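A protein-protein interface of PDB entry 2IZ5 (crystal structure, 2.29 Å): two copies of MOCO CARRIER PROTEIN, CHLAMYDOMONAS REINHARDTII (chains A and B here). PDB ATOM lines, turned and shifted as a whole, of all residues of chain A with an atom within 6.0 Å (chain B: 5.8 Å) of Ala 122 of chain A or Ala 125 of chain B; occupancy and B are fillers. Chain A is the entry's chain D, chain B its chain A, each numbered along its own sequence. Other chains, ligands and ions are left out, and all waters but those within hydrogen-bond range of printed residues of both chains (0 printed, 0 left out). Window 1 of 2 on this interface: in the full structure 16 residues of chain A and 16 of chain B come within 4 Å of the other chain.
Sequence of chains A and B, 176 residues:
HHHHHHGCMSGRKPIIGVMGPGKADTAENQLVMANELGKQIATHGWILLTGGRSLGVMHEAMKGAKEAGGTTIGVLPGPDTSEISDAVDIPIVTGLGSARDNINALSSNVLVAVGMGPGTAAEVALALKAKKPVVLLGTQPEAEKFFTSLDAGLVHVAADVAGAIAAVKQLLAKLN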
ATOM      1  N   ARG A 100       4.598  20.212  14.214  1.00  0.00           N
ATOM      2  CA  ARG A 100       5.279  19.235  15.055  1.00  0.00           C
ATOM      3  C   ARG A 100       5.590  19.814  16.431  1.00  0.00           C
ATOM      4  O   ARG A 100       6.602  20.491  16.615  1.00  0.00           O
ATOM      5  CB  ARG A 100       6.565  18.752  14.384  1.00  0.00           C
ATOM      6  CG  ARG A 100       6.669  17.241  14.254  1.00  0.00           C
ATOM      7  CD  ARG A 100       5.567  16.613  13.417  1.00  0.00           C
ATOM      8  NE  ARG A 100       5.061  15.380  14.014  1.00  0.00           N
ATOM      9  CZ  ARG A 100       3.855  15.250  14.550  1.00  0.00           C
ATOM     10  NH1 ARG A 100       3.021  16.281  14.566  1.00  0.00           N
ATOM     11  NH2 ARG A 100       3.480  14.091  15.071  1.00  0.00           N
ATOM     12  N   GLY A 117      -2.328   4.822  15.051  1.00  0.00           N
ATOM     13  CA  GLY A 117      -3.122   5.617  14.101  1.00  0.00           C
ATOM     14  C   GLY A 117      -2.109   6.487  13.400  1.00  0.00           C
ATOM     15  O   GLY A 117      -0.949   6.480  13.790  1.00  0.00           O
ATOM     16  N   PRO A 118      -2.505   7.220  12.348  1.00  0.00           N
ATOM     17  CA  PRO A 118      -1.521   8.075  11.624  1.00  0.00           C
ATOM     18  C   PRO A 118      -0.684   9.052  12.501  1.00  0.00           C
ATOM     19  O   PRO A 118       0.569   9.066  12.391  1.00  0.00           O
ATOM     20  CB  PRO A 118      -2.391   8.807  10.610  1.00  0.00           C
ATOM     21  CG  PRO A 118      -3.502   7.785  10.335  1.00  0.00           C
ATOM     22  CD  PRO A 118      -3.824   7.256  11.699  1.00  0.00           C
ATOM     23  N   GLY A 119      -1.376   9.821  13.356  1.00  0.00           N
ATOM     24  CA  GLY A 119      -0.740  10.721  14.282  1.00  0.00           C
ATOM     25  C   GLY A 119       0.355  10.076  15.105  1.00  0.00           C
ATOM     26  O   GLY A 119       1.473  10.569  15.152  1.00  0.00           O
ATOM     27  N   THR A 120       0.025   8.962  15.742  1.00  0.00           N
ATOM     28  CA  THR A 120       0.936   8.222  16.581  1.00  0.00           C
ATOM     29  C   THR A 120       2.120   7.617  15.806  1.00  0.00           C
ATOM     30  O   THR A 120       3.235   7.530  16.336  1.00  0.00           O
ATOM     31  CB  THR A 120       0.158   7.058  17.275  1.00  0.00           C
ATOM     32  OG1 THR A 120      -0.936   7.578  18.007  1.00  0.00           O
ATOM     33  CG2 THR A 120       1.014   6.265  18.237  1.00  0.00           C
ATOM     34  N   ALA A 121       1.860   7.125  14.595  1.00  0.00           N
ATOM     35  CA  ALA A 121       2.911   6.547  13.740  1.00  0.00           C
ATOM     36  C   ALA A 121       3.963   7.609  13.474  1.00  0.00           C
ATOM     37  O   ALA A 121       5.144   7.337  13.473  1.00  0.00           O
ATOM     38  CB  ALA A 121       2.320   6.031  12.412  1.00  0.00           C
ATOM     39  N   ALA A 122       3.502   8.822  13.251  1.00  0.00           N
ATOM     40  CA  ALA A 122       4.356   9.977  12.936  1.00  0.00           C
ATOM     41  C   ALA A 122       5.235  10.325  14.107  1.00  0.00           C
ATOM     42  O   ALA A 122       6.437  10.433  13.945  1.00  0.00           O
ATOM     43  CB  ALA A 122       3.503  11.178  12.512  1.00  0.00           C
ATOM     44  N   GLU A 123       4.636  10.384  15.296  1.00  0.00           N
ATOM     45  CA  GLU A 123       5.341  10.697  16.527  1.00  0.00           C
ATOM     46  C   GLU A 123       6.370   9.596  16.870  1.00  0.00           C
ATOM     47  O   GLU A 123       7.492   9.882  17.279  1.00  0.00           O
ATOM     48  CB  GLU A 123       4.346  10.935  17.672  1.00  0.00           C
ATOM     49  CG  GLU A 123       3.527  12.271  17.659  1.00  0.00           C
ATOM     50  CD  GLU A 123       2.439  12.423  18.833  1.00  0.00           C
ATOM     51  OE1 GLU A 123       2.669  12.114  20.039  1.00  0.00           O
ATOM     52  OE2 GLU A 123       1.305  12.892  18.548  1.00  0.00           O
ATOM     53  N   VAL A 124       6.029   8.330  16.666  1.00  0.00           N
ATOM     54  CA  VAL A 124       6.996   7.222  16.925  1.00  0.00           C
ATOM     55  C   VAL A 124       8.256   7.245  15.999  1.00  0.00           C
ATOM     56  O   VAL A 124       9.372   7.037  16.434  1.00  0.00           O
ATOM     57  CB  VAL A 124       6.295   5.871  16.813  1.00  0.00           C
ATOM     58  CG1 VAL A 124       7.305   4.738  16.816  1.00  0.00           C
ATOM     59  CG2 VAL A 124       5.208   5.732  17.941  1.00  0.00           C
ATOM     60  N   ALA A 125       8.035   7.524  14.733  1.00  0.00           N
ATOM     61  CA  ALA A 125       9.060   7.572  13.726  1.00  0.00           C
ATOM     62  C   ALA A 125      10.024   8.732  13.969  1.00  0.00           C
ATOM     63  O   ALA A 125      11.228   8.570  13.795  1.00  0.00           O
ATOM     64  CB  ALA A 125       8.403   7.668  12.368  1.00  0.00           C
ATOM     65  N   LEU A 126       9.499   9.889  14.391  1.00  0.00           N
ATOM     66  CA  LEU A 126      10.359  11.014  14.816  1.00  0.00           C
ATOM     67  C   LEU A 126      11.272  10.636  15.992  1.00  0.00           C
ATOM     68  O   LEU A 126      12.437  10.975  15.993  1.00  0.00           O
ATOM     69  CB  LEU A 126       9.550  12.223  15.273  1.00  0.00           C
ATOM     70  CG  LEU A 126       8.636  12.996  14.352  1.00  0.00           C
ATOM     71  CD1 LEU A 126       8.297  14.315  15.096  1.00  0.00           C
ATOM     72  CD2 LEU A 126       9.283  13.307  12.964  1.00  0.00           C
ATOM     73  N   ALA A 127      10.736   9.946  16.990  1.00  0.00           N
ATOM     74  CA  ALA A 127      11.528   9.539  18.138  1.00  0.00           C
ATOM     75  C   ALA A 127      12.653   8.629  17.727  1.00  0.00           C
ATOM     76  O   ALA A 127      13.806   8.880  18.068  1.00  0.00           O
ATOM     77  CB  ALA A 127      10.646   8.858  19.150  1.00  0.00           C
ATOM     78  N   PHE A 147       8.113  -0.852  12.639  1.00  0.00           N
ATOM     79  CA  PHE A 147       8.984   0.000  13.460  1.00  0.00           C
ATOM     80  C   PHE A 147      10.237  -0.750  13.851  1.00  0.00           C
ATOM     81  O   PHE A 147      11.316  -0.190  13.822  1.00  0.00           O
ATOM     82  CB  PHE A 147       8.240   0.603  14.666  1.00  0.00           C
ATOM     83  CG  PHE A 147       7.281   1.706  14.278  1.00  0.00           C
ATOM     84  CD1 PHE A 147       5.921   1.591  14.526  1.00  0.00           C
ATOM     85  CD2 PHE A 147       7.741   2.823  13.602  1.00  0.00           C
ATOM     86  CE1 PHE A 147       5.039   2.567  14.164  1.00  0.00           C
ATOM     87  CE2 PHE A 147       6.848   3.810  13.190  1.00  0.00           C
ATOM     88  CZ  PHE A 147       5.479   3.677  13.489  1.00  0.00           C
ATOM     89  N   THR B 120      11.347   9.396   6.506  1.00  0.00           N
ATOM     90  CA  THR B 120      10.342   9.206   5.501  1.00  0.00           C
ATOM     91  C   THR B 120       9.022   8.700   6.117  1.00  0.00           C
ATOM     92  O   THR B 120       7.954   9.164   5.752  1.00  0.00           O
ATOM     93  CB  THR B 120      10.810   8.206   4.422  1.00  0.00           C
ATOM     94  OG1 THR B 120      12.150   8.526   4.030  1.00  0.00           O
ATOM     95  CG2 THR B 120       9.808   8.237   3.198  1.00  0.00           C
ATOM     96  N   ALA B 121       9.145   7.719   7.012  1.00  0.00           N
ATOM     97  CA  ALA B 121       8.037   7.160   7.743  1.00  0.00           C
ATOM     98  C   ALA B 121       7.127   8.236   8.395  1.00  0.00           C
ATOM     99  O   ALA B 121       5.896   8.149   8.305  1.00  0.00           O
ATOM    100  CB  ALA B 121       8.567   6.138   8.774  1.00  0.00           C
ATOM    101  N   ALA B 122       7.724   9.233   9.037  1.00  0.00           N
ATOM    102  CA  ALA B 122       7.018  10.353   9.663  1.00  0.00           C
ATOM    103  C   ALA B 122       6.309  11.248   8.670  1.00  0.00           C
ATOM    104  O   ALA B 122       5.216  11.730   8.923  1.00  0.00           O
ATOM    105  CB  ALA B 122       8.022  11.204  10.433  1.00  0.00           C
ATOM    106  N   GLU B 123       6.986  11.559   7.579  1.00  0.00           N
ATOM    107  CA  GLU B 123       6.413  12.376   6.491  1.00  0.00           C
ATOM    108  C   GLU B 123       5.186  11.670   5.881  1.00  0.00           C
ATOM    109  O   GLU B 123       4.131  12.276   5.706  1.00  0.00           O
ATOM    110  CB  GLU B 123       7.459  12.646   5.389  1.00  0.00           C
ATOM    111  CG  GLU B 123       8.444  13.852   5.532  1.00  0.00           C
ATOM    112  CD  GLU B 123       9.517  13.839   4.369  1.00  0.00           C
ATOM    113  OE1 GLU B 123       9.798  12.752   3.838  1.00  0.00           O
ATOM    114  OE2 GLU B 123      10.079  14.873   3.950  1.00  0.00           O
ATOM    115  N   VAL B 124       5.343  10.409   5.522  1.00  0.00           N
ATOM    116  CA  VAL B 124       4.220   9.576   5.035  1.00  0.00           C
ATOM    117  C   VAL B 124       3.037   9.527   6.028  1.00  0.00           C
ATOM    118  O   VAL B 124       1.894   9.780   5.680  1.00  0.00           O
ATOM    119  CB  VAL B 124       4.667   8.143   4.763  1.00  0.00           C
ATOM    120  CG1 VAL B 124       3.499   7.270   4.330  1.00  0.00           C
ATOM    121  CG2 VAL B 124       5.743   8.118   3.717  1.00  0.00           C
ATOM    122  N   ALA B 125       3.307   9.211   7.274  1.00  0.00           N
ATOM    123  CA  ALA B 125       2.227   9.140   8.267  1.00  0.00           C
ATOM    124  C   ALA B 125       1.561  10.530   8.415  1.00  0.00           C
ATOM    125  O   ALA B 125       0.345  10.643   8.528  1.00  0.00           O
ATOM    126  CB  ALA B 125       2.788   8.646   9.575  1.00  0.00           C
ATOM    127  N   LEU B 126       2.358  11.602   8.378  1.00  0.00           N
ATOM    128  CA  LEU B 126       1.790  12.952   8.428  1.00  0.00           C
ATOM    129  C   LEU B 126       0.939  13.297   7.201  1.00  0.00           C
ATOM    130  O   LEU B 126      -0.085  13.952   7.320  1.00  0.00           O
ATOM    131  CB  LEU B 126       2.894  14.017   8.641  1.00  0.00           C
ATOM    132  CG  LEU B 126       3.470  14.094  10.046  1.00  0.00           C
ATOM    133  CD1 LEU B 126       4.763  14.916  10.076  1.00  0.00           C
ATOM    134  CD2 LEU B 126       2.448  14.651  11.013  1.00  0.00           C
ATOM    135  N   ALA B 127       1.340  12.865   6.033  1.00  0.00           N
ATOM    136  CA  ALA B 127       0.542  13.047   4.833  1.00  0.00           C
ATOM    137  C   ALA B 127      -0.783  12.296   4.916  1.00  0.00           C
ATOM    138  O   ALA B 127      -1.812  12.851   4.583  1.00  0.00           O
ATOM    139  CB  ALA B 127       1.316  12.599   3.634  1.00  0.00           C
ATOM    140  N   LEU B 128      -0.756  11.053   5.392  1.00  0.00           N
ATOM    141  CA  LEU B 128      -1.984  10.272   5.633  1.00  0.00           C
ATOM    142  C   LEU B 128      -2.859  10.839   6.759  1.00  0.00           C
ATOM    143  O   LEU B 128      -4.059  10.731   6.728  1.00  0.00           O
ATOM    144  CB  LEU B 128      -1.632   8.827   5.980  1.00  0.00           C
ATOM    145  CG  LEU B 128      -0.834   8.027   4.964  1.00  0.00           C
ATOM    146  CD1 LEU B 128      -0.370   6.684   5.591  1.00  0.00           C
ATOM    147  CD2 LEU B 128      -1.666   7.818   3.742  1.00  0.00           C
ATOM    148  N   LYS B 129      -2.231  11.414   7.772  1.00  0.00           N
ATOM    149  CA  LYS B 129      -2.939  12.151   8.807  1.00  0.00           C
ATOM    150  C   LYS B 129      -3.657  13.358   8.185  1.00  0.00           C
ATOM    151  O   LYS B 129      -4.785  13.597   8.492  1.00  0.00           O
ATOM    152  CB  LYS B 129      -1.932  12.520   9.910  1.00  0.00           C
ATOM    153  CG  LYS B 129      -2.277  13.607  10.908  1.00  0.00           C
ATOM    154  CD  LYS B 129      -3.239  13.182  11.912  1.00  0.00           C
ATOM    155  CE  LYS B 129      -3.533  14.373  12.840  1.00  0.00           C
ATOM    156  NZ  LYS B 129      -4.595  14.093  13.837  1.00  0.00           N
ATOM    157  N   ALA B 130      -3.019  14.067   7.269  1.00  0.00           N
ATOM    158  CA  ALA B 130      -3.668  15.130   6.502  1.00  0.00           C
ATOM    159  C   ALA B 130      -4.595  14.650   5.368  1.00  0.00           C
ATOM    160  O   ALA B 130      -5.111  15.474   4.611  1.00  0.00           O
ATOM    161  CB  ALA B 130      -2.601  16.091   5.919  1.00  0.00           C
ATOM    162  N   PHE B 147       1.450   0.981   6.306  1.00  0.00           N
ATOM    163  CA  PHE B 147       0.785   2.184   5.878  1.00  0.00           C
ATOM    164  C   PHE B 147      -0.568   1.880   5.291  1.00  0.00           C
ATOM    165  O   PHE B 147      -1.510   2.556   5.604  1.00  0.00           O
ATOM    166  CB  PHE B 147       1.676   2.993   4.925  1.00  0.00           C
ATOM    167  CG  PHE B 147       2.870   3.597   5.613  1.00  0.00           C
ATOM    168  CD1 PHE B 147       4.164   3.229   5.276  1.00  0.00           C
ATOM    169  CD2 PHE B 147       2.694   4.510   6.644  1.00  0.00           C
ATOM    170  CE1 PHE B 147       5.269   3.805   5.936  1.00  0.00           C
ATOM    171  CE2 PHE B 147       3.802   5.067   7.307  1.00  0.00           C
ATOM    172  CZ  PHE B 147       5.070   4.719   6.953  1.00  0.00           C
ATOM    173  N   LEU B 150      -2.833   1.611   8.109  1.00  0.00           N
ATOM    174  CA  LEU B 150      -3.281   2.947   8.564  1.00  0.00           C
ATOM    175  C   LEU B 150      -4.427   3.560   7.750  1.00  0.00           C
ATOM    176  O   LEU B 150      -5.421   4.052   8.328  1.00  0.00           O
ATOM    177  CB  LEU B 150      -2.124   3.955   8.576  1.00  0.00           C
ATOM    178  CG  LEU B 150      -1.025   3.769   9.599  1.00  0.00           C
ATOM    179  CD1 LEU B 150      -0.139   4.961   9.500  1.00  0.00           C
ATOM    180  CD2 LEU B 150      -1.578   3.595  10.996  1.00  0.00           C
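CD1 of Leu 126 of chain B touches CD of Arg 100 of chain A, at 3.8 Å.
Pro 118 of chain A touches Ala 125 of chain B (O to CB, 3.6 Å).
CB of Pro 118 of chain A touches CB of Lys 129 of chain B (3.8 Å).
CD2 of Leu 150 of chain B touches N of Pro 118 of chain A (3.98 Å).
Ala 121 of chain A touches Ala 125 of chain B.
Leu 150 of chain B touches Ala 121 of chain A.
Ala 122 of chain A touches Leu 126 of chain B (CB to CG, 3.8 Å).
CB of Ala 121 of chain B touches CB of Ala 125 of chain A, at 3.9 Å.
CB of Ala 125 of chain A touches N of Ala 122 of chain B, at 3.7 Å.
CD2 of Leu 126 of chain A touches CB of Ala 122 of chain B, at 3.5 Å.
Printed residues of chain A within 4 Å of Ala 121 of chain B: Ala 125 (3.9 Å).
Of the printed residues of chain B, Arg 100 of chain A touches Leu 126.
Of the printed residues of chain B, Leu 126 of chain A touches Ala 122 (3.5 Å).
The nearest residue of chain B that does not touch Ala 122 of chain A is Ala 121 of chain B (5.2 Å).
The nearest residue of chain A that does not touch Ala 125 of chain B is Gly 119 of chain A (5.2 Å).
The nearest printed residue of chain B that does not touch Gly 117 of chain A is Ala 125 of chain B (6.0 Å).
Ala 121 of chain A touches Ala 125 of chain B, and with the chains exchanged Ala 125 of chain A touches Ala 121 of chain B.
Ala 122 of chain B touches its own counterpart, Ala 122 of chain A.
Ala 122 of chain A touches Ala 125 of chain B, and with the chains exchanged Ala 125 of chain A touches Ala 122 of chain B.
Ala 122 of chain A touches Leu 126 of chain B, and with the chains exchanged Leu 126 of chain A touches Ala 122 of chain B.
Of the 13 pairs that touch across the chains among the printed residues, 7 have their exchanged pair printed and touching as well.
Hydrophobic or aromatic side chains of chain A that line the printed part of chain B: Pro 118, Ala 121, Ala 122, Ala 125 and Leu 126.
Of the 13 printed residues of chain B, 6 touch a printed residue of chain A.
Printed residues of chain B that touch a printed residue of chain A: Ala 121, Ala 122, Ala 125, Leu 126, Lys 129 and Leu 150.
Hydrophobic or aromatic side chains of chain B that line the printed part of chain A: Ala 121, Ala 122, Ala 125, Leu 126 and Leu 150.
Among the printed residues, 13 pairs touch across the chains.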
